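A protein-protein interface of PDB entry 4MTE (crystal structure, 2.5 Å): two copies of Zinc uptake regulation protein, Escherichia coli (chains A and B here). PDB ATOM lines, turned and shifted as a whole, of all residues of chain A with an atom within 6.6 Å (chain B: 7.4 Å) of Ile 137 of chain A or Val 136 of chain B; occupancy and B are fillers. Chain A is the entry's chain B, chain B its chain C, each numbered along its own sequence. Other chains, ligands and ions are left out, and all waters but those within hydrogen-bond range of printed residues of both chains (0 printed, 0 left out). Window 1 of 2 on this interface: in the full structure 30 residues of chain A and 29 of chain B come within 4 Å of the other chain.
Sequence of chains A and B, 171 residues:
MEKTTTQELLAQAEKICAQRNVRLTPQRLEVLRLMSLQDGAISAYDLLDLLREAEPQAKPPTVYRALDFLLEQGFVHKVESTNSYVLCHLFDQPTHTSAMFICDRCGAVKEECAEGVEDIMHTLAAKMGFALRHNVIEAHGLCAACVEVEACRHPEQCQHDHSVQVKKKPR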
ATOM      1  N   GLU A  80      -0.092 -24.285  -0.500  1.00  0.00           N
ATOM      2  CA  GLU A  80      -0.203 -22.830  -0.471  1.00  0.00           C
ATOM      3  C   GLU A  80      -1.118 -22.287  -1.561  1.00  0.00           C
ATOM      4  O   GLU A  80      -1.835 -21.309  -1.347  1.00  0.00           O
ATOM      5  CB  GLU A  80       1.188 -22.206  -0.608  1.00  0.00           C
ATOM      6  CG  GLU A  80       2.159 -22.607   0.497  1.00  0.00           C
ATOM      7  CD  GLU A  80       1.874 -21.914   1.819  1.00  0.00           C
ATOM      8  OE1 GLU A  80       0.920 -21.110   1.886  1.00  0.00           O
ATOM      9  OE2 GLU A  80       2.612 -22.175   2.793  1.00  0.00           O
ATOM     10  N   SER A  81      -1.098 -22.922  -2.729  1.00  0.00           N
ATOM     11  CA  SER A  81      -1.827 -22.404  -3.884  1.00  0.00           C
ATOM     12  C   SER A  81      -3.328 -22.658  -3.784  1.00  0.00           C
ATOM     13  O   SER A  81      -4.117 -22.025  -4.490  1.00  0.00           O
ATOM     14  CB  SER A  81      -1.276 -23.008  -5.177  1.00  0.00           C
ATOM     15  OG  SER A  81      -1.414 -24.417  -5.184  1.00  0.00           O
ATOM     16  N   THR A  97      11.948 -31.404   0.970  1.00  0.00           N
ATOM     17  CA  THR A  97      11.369 -30.627  -0.113  1.00  0.00           C
ATOM     18  C   THR A  97      10.514 -31.561  -0.957  1.00  0.00           C
ATOM     19  O   THR A  97      11.021 -32.524  -1.535  1.00  0.00           O
ATOM     20  CB  THR A  97      12.464 -29.995  -0.988  1.00  0.00           C
ATOM     21  OG1 THR A  97      13.359 -29.240  -0.163  1.00  0.00           O
ATOM     22  CG2 THR A  97      11.859 -29.086  -2.049  1.00  0.00           C
ATOM     23  N   SER A  98       9.221 -31.266  -1.024  1.00  0.00           N
ATOM     24  CA  SER A  98       8.260 -32.150  -1.668  1.00  0.00           C
ATOM     25  C   SER A  98       7.547 -31.440  -2.809  1.00  0.00           C
ATOM     26  O   SER A  98       7.125 -30.293  -2.669  1.00  0.00           O
ATOM     27  CB  SER A  98       7.229 -32.629  -0.646  1.00  0.00           C
ATOM     28  OG  SER A  98       6.237 -31.641  -0.431  1.00  0.00           O
ATOM     29  N   ALA A  99       7.411 -32.129  -3.937  1.00  0.00           N
ATOM     30  CA  ALA A  99       6.669 -31.599  -5.074  1.00  0.00           C
ATOM     31  C   ALA A  99       5.220 -32.072  -4.994  1.00  0.00           C
ATOM     32  O   ALA A  99       4.957 -33.246  -4.736  1.00  0.00           O
ATOM     33  CB  ALA A  99       7.310 -32.039  -6.383  1.00  0.00           C
ATOM     34  N   MET A 100       4.291 -31.145  -5.211  1.00  0.00           N
ATOM     35  CA  MET A 100       2.866 -31.411  -5.054  1.00  0.00           C
ATOM     36  C   MET A 100       2.150 -31.301  -6.385  1.00  0.00           C
ATOM     37  O   MET A 100       2.174 -30.252  -7.026  1.00  0.00           O
ATOM     38  CB  MET A 100       2.253 -30.415  -4.065  1.00  0.00           C
ATOM     39  CG  MET A 100       2.703 -30.628  -2.634  1.00  0.00           C
ATOM     40  SD  MET A 100       1.905 -32.053  -1.874  1.00  0.00           S
ATOM     41  CE  MET A 100       3.056 -32.425  -0.558  1.00  0.00           C
ATOM     42  N   PHE A 101       1.510 -32.391  -6.792  1.00  0.00           N
ATOM     43  CA  PHE A 101       0.727 -32.404  -8.015  1.00  0.00           C
ATOM     44  C   PHE A 101      -0.748 -32.399  -7.662  1.00  0.00           C
ATOM     45  O   PHE A 101      -1.255 -33.327  -7.031  1.00  0.00           O
ATOM     46  CB  PHE A 101       1.104 -33.605  -8.872  1.00  0.00           C
ATOM     47  CG  PHE A 101       2.512 -33.542  -9.385  1.00  0.00           C
ATOM     48  CD1 PHE A 101       2.775 -33.139 -10.682  1.00  0.00           C
ATOM     49  CD2 PHE A 101       3.576 -33.851  -8.557  1.00  0.00           C
ATOM     50  CE1 PHE A 101       4.071 -33.069 -11.149  1.00  0.00           C
ATOM     51  CE2 PHE A 101       4.874 -33.781  -9.020  1.00  0.00           C
ATOM     52  CZ  PHE A 101       5.121 -33.390 -10.316  1.00  0.00           C
ATOM     53  N   ALA A 114      11.893 -34.859  -4.914  1.00  0.00           N
ATOM     54  CA  ALA A 114      12.646 -34.272  -6.017  1.00  0.00           C
ATOM     55  C   ALA A 114      13.865 -33.539  -5.465  1.00  0.00           C
ATOM     56  O   ALA A 114      13.886 -32.311  -5.389  1.00  0.00           O
ATOM     57  CB  ALA A 114      11.763 -33.330  -6.829  1.00  0.00           C
ATOM     58  N   VAL A 117      15.524 -30.728  -7.408  1.00  0.00           N
ATOM     59  CA  VAL A 117      14.916 -29.407  -7.273  1.00  0.00           C
ATOM     60  C   VAL A 117      15.536 -28.633  -6.115  1.00  0.00           C
ATOM     61  O   VAL A 117      15.908 -27.470  -6.271  1.00  0.00           O
ATOM     62  CB  VAL A 117      13.390 -29.508  -7.061  1.00  0.00           C
ATOM     63  CG1 VAL A 117      12.763 -28.122  -6.906  1.00  0.00           C
ATOM     64  CG2 VAL A 117      12.748 -30.259  -8.219  1.00  0.00           C
ATOM     65  N   GLU A 118      15.638 -29.281  -4.957  1.00  0.00           N
ATOM     66  CA  GLU A 118      16.293 -28.684  -3.797  1.00  0.00           C
ATOM     67  C   GLU A 118      17.681 -28.205  -4.200  1.00  0.00           C
ATOM     68  O   GLU A 118      18.053 -27.061  -3.930  1.00  0.00           O
ATOM     69  CB  GLU A 118      16.397 -29.696  -2.652  1.00  0.00           C
ATOM     70  CG  GLU A 118      17.195 -29.213  -1.437  1.00  0.00           C
ATOM     71  CD  GLU A 118      16.523 -28.071  -0.697  1.00  0.00           C
ATOM     72  OE1 GLU A 118      15.296 -27.901  -0.845  1.00  0.00           O
ATOM     73  OE2 GLU A 118      17.224 -27.341   0.037  1.00  0.00           O
ATOM     74  N   MET A 121      17.475 -25.126  -6.659  1.00  0.00           N
ATOM     75  CA  MET A 121      17.028 -23.946  -5.927  1.00  0.00           C
ATOM     76  C   MET A 121      18.112 -23.446  -4.978  1.00  0.00           C
ATOM     77  O   MET A 121      18.301 -22.241  -4.819  1.00  0.00           O
ATOM     78  CB  MET A 121      15.756 -24.266  -5.142  1.00  0.00           C
ATOM     79  CG  MET A 121      14.554 -24.580  -6.015  1.00  0.00           C
ATOM     80  SD  MET A 121      13.976 -23.157  -6.954  1.00  0.00           S
ATOM     81  CE  MET A 121      13.271 -22.139  -5.661  1.00  0.00           C
ATOM     82  N   ASN A 135      11.205 -24.458   0.386  1.00  0.00           N
ATOM     83  CA  ASN A 135      10.737 -24.338  -0.987  1.00  0.00           C
ATOM     84  C   ASN A 135       9.249 -24.653  -1.059  1.00  0.00           C
ATOM     85  O   ASN A 135       8.739 -25.471  -0.293  1.00  0.00           O
ATOM     86  CB  ASN A 135      11.518 -25.278  -1.908  1.00  0.00           C
ATOM     87  CG  ASN A 135      12.985 -24.906  -2.018  1.00  0.00           C
ATOM     88  OD1 ASN A 135      13.856 -25.636  -1.550  1.00  0.00           O
ATOM     89  ND2 ASN A 135      13.264 -23.769  -2.644  1.00  0.00           N
ATOM     90  N   VAL A 136       8.560 -23.987  -1.979  1.00  0.00           N
ATOM     91  CA  VAL A 136       7.151 -24.245  -2.238  1.00  0.00           C
ATOM     92  C   VAL A 136       7.013 -24.614  -3.708  1.00  0.00           C
ATOM     93  O   VAL A 136       7.160 -23.765  -4.588  1.00  0.00           O
ATOM     94  CB  VAL A 136       6.281 -23.016  -1.921  1.00  0.00           C
ATOM     95  CG1 VAL A 136       4.812 -23.297  -2.232  1.00  0.00           C
ATOM     96  CG2 VAL A 136       6.466 -22.595  -0.465  1.00  0.00           C
ATOM     97  N   ILE A 137       6.740 -25.889  -3.962  1.00  0.00           N
ATOM     98  CA  ILE A 137       6.718 -26.431  -5.316  1.00  0.00           C
ATOM     99  C   ILE A 137       5.418 -27.179  -5.542  1.00  0.00           C
ATOM    100  O   ILE A 137       5.238 -28.296  -5.056  1.00  0.00           O
ATOM    101  CB  ILE A 137       7.908 -27.380  -5.545  1.00  0.00           C
ATOM    102  CG1 ILE A 137       9.224 -26.612  -5.413  1.00  0.00           C
ATOM    103  CG2 ILE A 137       7.826 -28.043  -6.917  1.00  0.00           C
ATOM    104  CD1 ILE A 137      10.305 -27.383  -4.693  1.00  0.00           C
ATOM    105  N   GLU A 138       4.516 -26.553  -6.288  1.00  0.00           N
ATOM    106  CA  GLU A 138       3.178 -27.084  -6.481  1.00  0.00           C
ATOM    107  C   GLU A 138       2.796 -27.005  -7.954  1.00  0.00           C
ATOM    108  O   GLU A 138       2.888 -25.949  -8.576  1.00  0.00           O
ATOM    109  CB  GLU A 138       2.186 -26.307  -5.615  1.00  0.00           C
ATOM    110  CG  GLU A 138       2.593 -26.261  -4.147  1.00  0.00           C
ATOM    111  CD  GLU A 138       1.664 -25.430  -3.286  1.00  0.00           C
ATOM    112  OE1 GLU A 138       0.818 -24.699  -3.841  1.00  0.00           O
ATOM    113  OE2 GLU A 138       1.786 -25.511  -2.046  1.00  0.00           O
ATOM    114  N   ALA A 139       2.380 -28.140  -8.499  1.00  0.00           N
ATOM    115  CA  ALA A 139       2.007 -28.246  -9.899  1.00  0.00           C
ATOM    116  C   ALA A 139       0.499 -28.417 -10.004  1.00  0.00           C
ATOM    117  O   ALA A 139      -0.103 -29.150  -9.220  1.00  0.00           O
ATOM    118  CB  ALA A 139       2.723 -29.422 -10.537  1.00  0.00           C
ATOM    119  N   HIS A 140      -0.104 -27.733 -10.972  1.00  0.00           N
ATOM    120  CA  HIS A 140      -1.547 -27.786 -11.179  1.00  0.00           C
ATOM    121  C   HIS A 140      -1.877 -28.349 -12.551  1.00  0.00           C
ATOM    122  O   HIS A 140      -1.217 -28.032 -13.538  1.00  0.00           O
ATOM    123  CB  HIS A 140      -2.155 -26.392 -11.028  1.00  0.00           C
ATOM    124  CG  HIS A 140      -2.261 -25.940  -9.608  1.00  0.00           C
ATOM    125  ND1 HIS A 140      -3.379 -26.172  -8.836  1.00  0.00           N
ATOM    126  CD2 HIS A 140      -1.382 -25.290  -8.812  1.00  0.00           C
ATOM    127  CE1 HIS A 140      -3.187 -25.674  -7.628  1.00  0.00           C
ATOM    128  NE2 HIS A 140      -1.983 -25.133  -7.586  1.00  0.00           N
ATOM    129  N   LYS B  78       1.090 -13.836  -9.257  1.00  0.00           N
ATOM    130  CA  LYS B  78       0.599 -14.027  -7.905  1.00  0.00           C
ATOM    131  C   LYS B  78       1.630 -14.801  -7.098  1.00  0.00           C
ATOM    132  O   LYS B  78       2.162 -15.809  -7.559  1.00  0.00           O
ATOM    133  CB  LYS B  78      -0.729 -14.783  -7.899  1.00  0.00           C
ATOM    134  CG  LYS B  78      -1.257 -15.020  -6.493  1.00  0.00           C
ATOM    135  CD  LYS B  78      -2.733 -15.365  -6.487  1.00  0.00           C
ATOM    136  CE  LYS B  78      -3.295 -15.374  -5.072  1.00  0.00           C
ATOM    137  NZ  LYS B  78      -4.779 -15.504  -5.058  1.00  0.00           N
ATOM    138  N   VAL B  79       1.914 -14.318  -5.896  1.00  0.00           N
ATOM    139  CA  VAL B  79       2.740 -15.060  -4.954  1.00  0.00           C
ATOM    140  C   VAL B  79       1.792 -15.824  -4.033  1.00  0.00           C
ATOM    141  O   VAL B  79       1.198 -15.248  -3.121  1.00  0.00           O
ATOM    142  CB  VAL B  79       3.652 -14.129  -4.135  1.00  0.00           C
ATOM    143  CG1 VAL B  79       4.714 -14.942  -3.402  1.00  0.00           C
ATOM    144  CG2 VAL B  79       4.294 -13.069  -5.040  1.00  0.00           C
ATOM    145  N   GLU B  80       1.643 -17.120  -4.294  1.00  0.00           N
ATOM    146  CA  GLU B  80       0.621 -17.931  -3.636  1.00  0.00           C
ATOM    147  C   GLU B  80       0.861 -18.072  -2.133  1.00  0.00           C
ATOM    148  O   GLU B  80      -0.089 -18.107  -1.353  1.00  0.00           O
ATOM    149  CB  GLU B  80       0.549 -19.317  -4.290  1.00  0.00           C
ATOM    150  CG  GLU B  80       0.109 -19.300  -5.758  1.00  0.00           C
ATOM    151  CD  GLU B  80      -1.378 -19.037  -5.938  1.00  0.00           C
ATOM    152  OE1 GLU B  80      -2.107 -18.956  -4.926  1.00  0.00           O
ATOM    153  OE2 GLU B  80      -1.820 -18.914  -7.100  1.00  0.00           O
ATOM    154  N   SER B  81       2.127 -18.130  -1.730  1.00  0.00           N
ATOM    155  CA  SER B  81       2.475 -18.415  -0.338  1.00  0.00           C
ATOM    156  C   SER B  81       2.470 -17.169   0.553  1.00  0.00           C
ATOM    157  O   SER B  81       2.813 -17.246   1.734  1.00  0.00           O
ATOM    158  CB  SER B  81       3.844 -19.096  -0.264  1.00  0.00           C
ATOM    159  OG  SER B  81       4.878 -18.219  -0.670  1.00  0.00           O
ATOM    160  N   THR B  97       7.684 -19.083 -16.689  1.00  0.00           N
ATOM    161  CA  THR B  97       7.325 -19.571 -15.366  1.00  0.00           C
ATOM    162  C   THR B  97       8.330 -19.029 -14.361  1.00  0.00           C
ATOM    163  O   THR B  97       9.518 -19.345 -14.420  1.00  0.00           O
ATOM    164  CB  THR B  97       7.324 -21.106 -15.316  1.00  0.00           C
ATOM    165  OG1 THR B  97       6.378 -21.617 -16.263  1.00  0.00           O
ATOM    166  CG2 THR B  97       6.975 -21.613 -13.919  1.00  0.00           C
ATOM    167  N   SER B  98       7.837 -18.215 -13.436  1.00  0.00           N
ATOM    168  CA  SER B  98       8.683 -17.533 -12.468  1.00  0.00           C
ATOM    169  C   SER B  98       8.981 -18.414 -11.261  1.00  0.00           C
ATOM    170  O   SER B  98       8.133 -19.195 -10.827  1.00  0.00           O
ATOM    171  CB  SER B  98       7.996 -16.252 -11.997  1.00  0.00           C
ATOM    172  OG  SER B  98       6.740 -16.547 -11.410  1.00  0.00           O
ATOM    173  N   ALA B  99      10.193 -18.287 -10.732  1.00  0.00           N
ATOM    174  CA  ALA B  99      10.553 -18.868  -9.445  1.00  0.00           C
ATOM    175  C   ALA B  99      10.797 -17.713  -8.478  1.00  0.00           C
ATOM    176  O   ALA B  99      11.785 -16.991  -8.612  1.00  0.00           O
ATOM    177  CB  ALA B  99      11.795 -19.741  -9.575  1.00  0.00           C
ATOM    178  N   MET B 100       9.897 -17.531  -7.512  1.00  0.00           N
ATOM    179  CA  MET B 100       9.928 -16.337  -6.660  1.00  0.00           C
ATOM    180  C   MET B 100      10.698 -16.558  -5.368  1.00  0.00           C
ATOM    181  O   MET B 100      10.310 -17.379  -4.547  1.00  0.00           O
ATOM    182  CB  MET B 100       8.506 -15.887  -6.311  1.00  0.00           C
ATOM    183  CG  MET B 100       7.720 -15.329  -7.482  1.00  0.00           C
ATOM    184  SD  MET B 100       8.499 -13.886  -8.220  1.00  0.00           S
ATOM    185  CE  MET B 100       7.258 -13.400  -9.409  1.00  0.00           C
ATOM    186  N   VAL B 117      13.859 -26.935 -12.773  1.00  0.00           N
ATOM    187  CA  VAL B 117      12.776 -27.350 -11.889  1.00  0.00           C
ATOM    188  C   VAL B 117      11.545 -27.704 -12.716  1.00  0.00           C
ATOM    189  O   VAL B 117      10.910 -28.733 -12.490  1.00  0.00           O
ATOM    190  CB  VAL B 117      12.431 -26.239 -10.858  1.00  0.00           C
ATOM    191  CG1 VAL B 117      11.251 -26.651  -9.971  1.00  0.00           C
ATOM    192  CG2 VAL B 117      13.655 -25.910 -10.009  1.00  0.00           C
ATOM    193  N   MET B 121       9.732 -31.230 -13.083  1.00  0.00           N
ATOM    194  CA  MET B 121       8.302 -31.305 -12.797  1.00  0.00           C
ATOM    195  C   MET B 121       7.565 -31.975 -13.956  1.00  0.00           C
ATOM    196  O   MET B 121       6.694 -32.820 -13.744  1.00  0.00           O
ATOM    197  CB  MET B 121       7.731 -29.904 -12.549  1.00  0.00           C
ATOM    198  CG  MET B 121       6.856 -29.778 -11.302  1.00  0.00           C
ATOM    199  SD  MET B 121       7.636 -30.337  -9.770  1.00  0.00           S
ATOM    200  CE  MET B 121       9.259 -29.590  -9.859  1.00  0.00           C
ATOM    201  N   LEU B 132       0.311 -31.539 -16.904  1.00  0.00           N
ATOM    202  CA  LEU B 132       0.792 -30.367 -16.173  1.00  0.00           C
ATOM    203  C   LEU B 132       0.423 -29.067 -16.889  1.00  0.00           C
ATOM    204  O   LEU B 132       0.871 -28.818 -18.006  1.00  0.00           O
ATOM    205  CB  LEU B 132       2.306 -30.461 -15.978  1.00  0.00           C
ATOM    206  CG  LEU B 132       2.997 -29.366 -15.164  1.00  0.00           C
ATOM    207  CD1 LEU B 132       2.116 -28.848 -14.037  1.00  0.00           C
ATOM    208  CD2 LEU B 132       4.304 -29.913 -14.608  1.00  0.00           C
ATOM    209  N   HIS B 134       0.303 -25.801 -15.111  1.00  0.00           N
ATOM    210  CA  HIS B 134       1.038 -24.672 -14.546  1.00  0.00           C
ATOM    211  C   HIS B 134       1.775 -25.067 -13.271  1.00  0.00           C
ATOM    212  O   HIS B 134       1.261 -25.835 -12.456  1.00  0.00           O
ATOM    213  CB  HIS B 134       0.092 -23.506 -14.255  1.00  0.00           C
ATOM    214  CG  HIS B 134       0.795 -22.247 -13.858  1.00  0.00           C
ATOM    215  ND1 HIS B 134       0.872 -21.816 -12.549  1.00  0.00           N
ATOM    216  CD2 HIS B 134       1.463 -21.326 -14.594  1.00  0.00           C
ATOM    217  CE1 HIS B 134       1.550 -20.685 -12.500  1.00  0.00           C
ATOM    218  NE2 HIS B 134       1.921 -20.365 -13.726  1.00  0.00           N
ATOM    219  N   ASN B 135       2.981 -24.530 -13.110  1.00  0.00           N
ATOM    220  CA  ASN B 135       3.796 -24.773 -11.925  1.00  0.00           C
ATOM    221  C   ASN B 135       3.895 -23.542 -11.033  1.00  0.00           C
ATOM    222  O   ASN B 135       3.905 -22.410 -11.514  1.00  0.00           O
ATOM    223  CB  ASN B 135       5.205 -25.212 -12.330  1.00  0.00           C
ATOM    224  CG  ASN B 135       5.279 -26.676 -12.700  1.00  0.00           C
ATOM    225  OD1 ASN B 135       4.619 -27.516 -12.092  1.00  0.00           O
ATOM    226  ND2 ASN B 135       6.095 -26.993 -13.697  1.00  0.00           N
ATOM    227  N   VAL B 136       3.972 -23.786  -9.729  1.00  0.00           N
ATOM    228  CA  VAL B 136       4.218 -22.743  -8.747  1.00  0.00           C
ATOM    229  C   VAL B 136       5.554 -23.045  -8.092  1.00  0.00           C
ATOM    230  O   VAL B 136       5.749 -24.133  -7.550  1.00  0.00           O
ATOM    231  CB  VAL B 136       3.108 -22.699  -7.679  1.00  0.00           C
ATOM    232  CG1 VAL B 136       3.453 -21.695  -6.571  1.00  0.00           C
ATOM    233  CG2 VAL B 136       1.769 -22.363  -8.329  1.00  0.00           C
ATOM    234  N   ILE B 137       6.475 -22.088  -8.164  1.00  0.00           N
ATOM    235  CA  ILE B 137       7.807 -22.253  -7.592  1.00  0.00           C
ATOM    236  C   ILE B 137       8.174 -21.028  -6.757  1.00  0.00           C
ATOM    237  O   ILE B 137       8.370 -19.924  -7.279  1.00  0.00           O
ATOM    238  CB  ILE B 137       8.869 -22.504  -8.683  1.00  0.00           C
ATOM    239  CG1 ILE B 137       8.391 -23.600  -9.643  1.00  0.00           C
ATOM    240  CG2 ILE B 137      10.204 -22.887  -8.042  1.00  0.00           C
ATOM    241  CD1 ILE B 137       9.314 -23.858 -10.819  1.00  0.00           C
ATOM    242  N   GLU B 138       8.251 -21.240  -5.449  1.00  0.00           N
ATOM    243  CA  GLU B 138       8.483 -20.161  -4.500  1.00  0.00           C
ATOM    244  C   GLU B 138       9.434 -20.606  -3.398  1.00  0.00           C
ATOM    245  O   GLU B 138       9.336 -21.720  -2.886  1.00  0.00           O
ATOM    246  CB  GLU B 138       7.155 -19.697  -3.901  1.00  0.00           C
ATOM    247  CG  GLU B 138       6.223 -19.051  -4.910  1.00  0.00           C
ATOM    248  CD  GLU B 138       4.862 -18.725  -4.333  1.00  0.00           C
ATOM    249  OE1 GLU B 138       4.688 -18.856  -3.104  1.00  0.00           O
ATOM    250  OE2 GLU B 138       3.964 -18.336  -5.109  1.00  0.00           O
ATOM    251  N   ALA B 139      10.359 -19.718  -3.052  1.00  0.00           N
ATOM    252  CA  ALA B 139      11.340 -19.966  -2.009  1.00  0.00           C
ATOM    253  C   ALA B 139      11.185 -18.913  -0.918  1.00  0.00           C
ATOM    254  O   ALA B 139      10.932 -17.742  -1.203  1.00  0.00           O
ATOM    255  CB  ALA B 139      12.742 -19.925  -2.591  1.00  0.00           C
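N of Val 136 of chain B is in hydrogen-bond range of O of Glu 138 of chain A (2.7 Å). N of Val 136 of chain A sits at hydrogen-bond distance from O of Glu 138 of chain B, at 2.6 Å. O of Val 136 of chain B sits close to O of Val 136 of chain A (3.3 Å). The backbone NH (N) of His 140 of chain A sits at hydrogen-bond distance from the backbone carbonyl oxygen (O) of His 134 of chain B (2.8 Å).
The backbone NH (N) of Ala 139 of chain B lies within hydrogen-bond range of the backbone carbonyl oxygen (O) of Met 100 of chain B, at 2.8 Å. The backbone carbonyl oxygen of Ile 137 of chain B sits at hydrogen-bond distance from the backbone NH of Met 100 of chain B, at 2.8 Å. The side-chain hydroxyl of Ser 81 of chain A lies within hydrogen-bond range of the side-chain carboxylate of Glu 138 of chain A (2.6 Å). The side-chain carboxylate (OE2) of Glu 138 of chain A sits at hydrogen-bond distance from the backbone NH (N) of Glu 80 of chain A (2.7 Å). OE1 of Glu 138 of chain B is in hydrogen-bond range of OG of Ser 81 of chain B (2.5 Å). O of Met 100 of chain A is in hydrogen-bond range of N of Ala 139 of chain A, 2.6 Å away.
Among the printed residues, merely in contact across the chains: Ala 139 of chain A with Asn 135 of chain B (3.1 Å), Ile 137 of chain A with Val 136 of chain B (3.3 Å), Val 136 of chain A with Ile 137 of chain B (3.4 Å), Asn 135 of chain A with Glu 138 of chain B (3.5 Å), His 140 of chain A with Leu 132 of chain B (3.5 Å), Glu 138 of chain A with Asn 135 of chain B (3.6 Å), Ala 139 of chain A with His 134 of chain B (3.6 Å), Ala 139 of chain A with Leu 132 of chain B (3.6 Å), Ser 81 of chain A with Glu 80 of chain B (3.6 Å), Ile 137 of chain A with Met 121 of chain B (3.6 Å), Glu 80 of chain A with Glu 80 of chain B (3.6 Å), Phe 101 of chain A with Met 121 of chain B (3.7 Å), Val 117 of chain A with Val 117 of chain B (3.7 Å), Ala 99 of chain A with Met 121 of chain B (3.8 Å), Met 121 of chain A with Ala 139 of chain B (3.8 Å), Glu 80 of chain A with Ser 81 of chain B (3.8 Å), Asn 135 of chain A with Ala 139 of chain B (3.9 Å), Val 117 of chain A with Met 121 of chain B (3.9 Å) and Met 121 of chain A with Ile 137 of chain B (3.9 Å).
Of the printed residues of chain A, Asn 135 of chain B touches Glu 138 and Ala 139. Of the printed residues of chain B, Met 121 of chain A touches Ile 137 (3.9 Å) and Ala 139 (3.8 Å). Printed residues of chain B within 4 Å of Ala 139 of chain A: Leu 132 (3.6 Å), His 134 (3.6 Å) and Asn 135 (3.1 Å). Printed residues of chain A within 4 Å of His 134 of chain B: Ala 139 and His 140. Printed residues of chain B within 4 Å of Asn 135 of chain A: Glu 138 and Ala 139. Ser 98 of chain B touches none of the printed residues of chain A. Thr 97 of chain A touches none of the printed residues of chain B. The nearest residue of chain B that does not touch Ile 137 of chain A is Ile 137 of chain B (4.7 Å).
Hydrophobic or aromatic side chains of chain A that line the printed part of chain B: Ala 99, Phe 101, Val 117, Met 121, Val 136, Ile 137, Ala 139 and His 140. Of the 17 printed residues of chain B, 11 touch a printed residue of chain A. Hydrophobic or aromatic side chains of chain B that line the printed part of chain A: Val 117, Met 121, Leu 132, Val 136, Ile 137 and Ala 139. Among the printed residues, 23 pairs touch across the chains. Among the printed residues, no Asp or Glu carboxylate lies within 4 Å of a Lys or Arg side-chain nitrogen of the other chain.
Glu 80 of chain A touches Ser 81 of chain B, and with the chains exchanged Ser 81 of chain A touches Glu 80 of chain B. Met 121 of chain A touches Ile 137 of chain B, and with the chains exchanged Ile 137 of chain A touches Met 121 of chain B. Asn 135 of chain A touches Glu 138 of chain B, and with the chains exchanged Glu 138 of chain A touches Asn 135 of chain B. Val 136 of chain A touches Glu 138 of chain B, and with the chains exchanged Glu 138 of chain A touches Val 136 of chain B. Of the 23 pairs that touch across the chains among the printed residues, 15 have their exchanged pair printed and touching as well.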
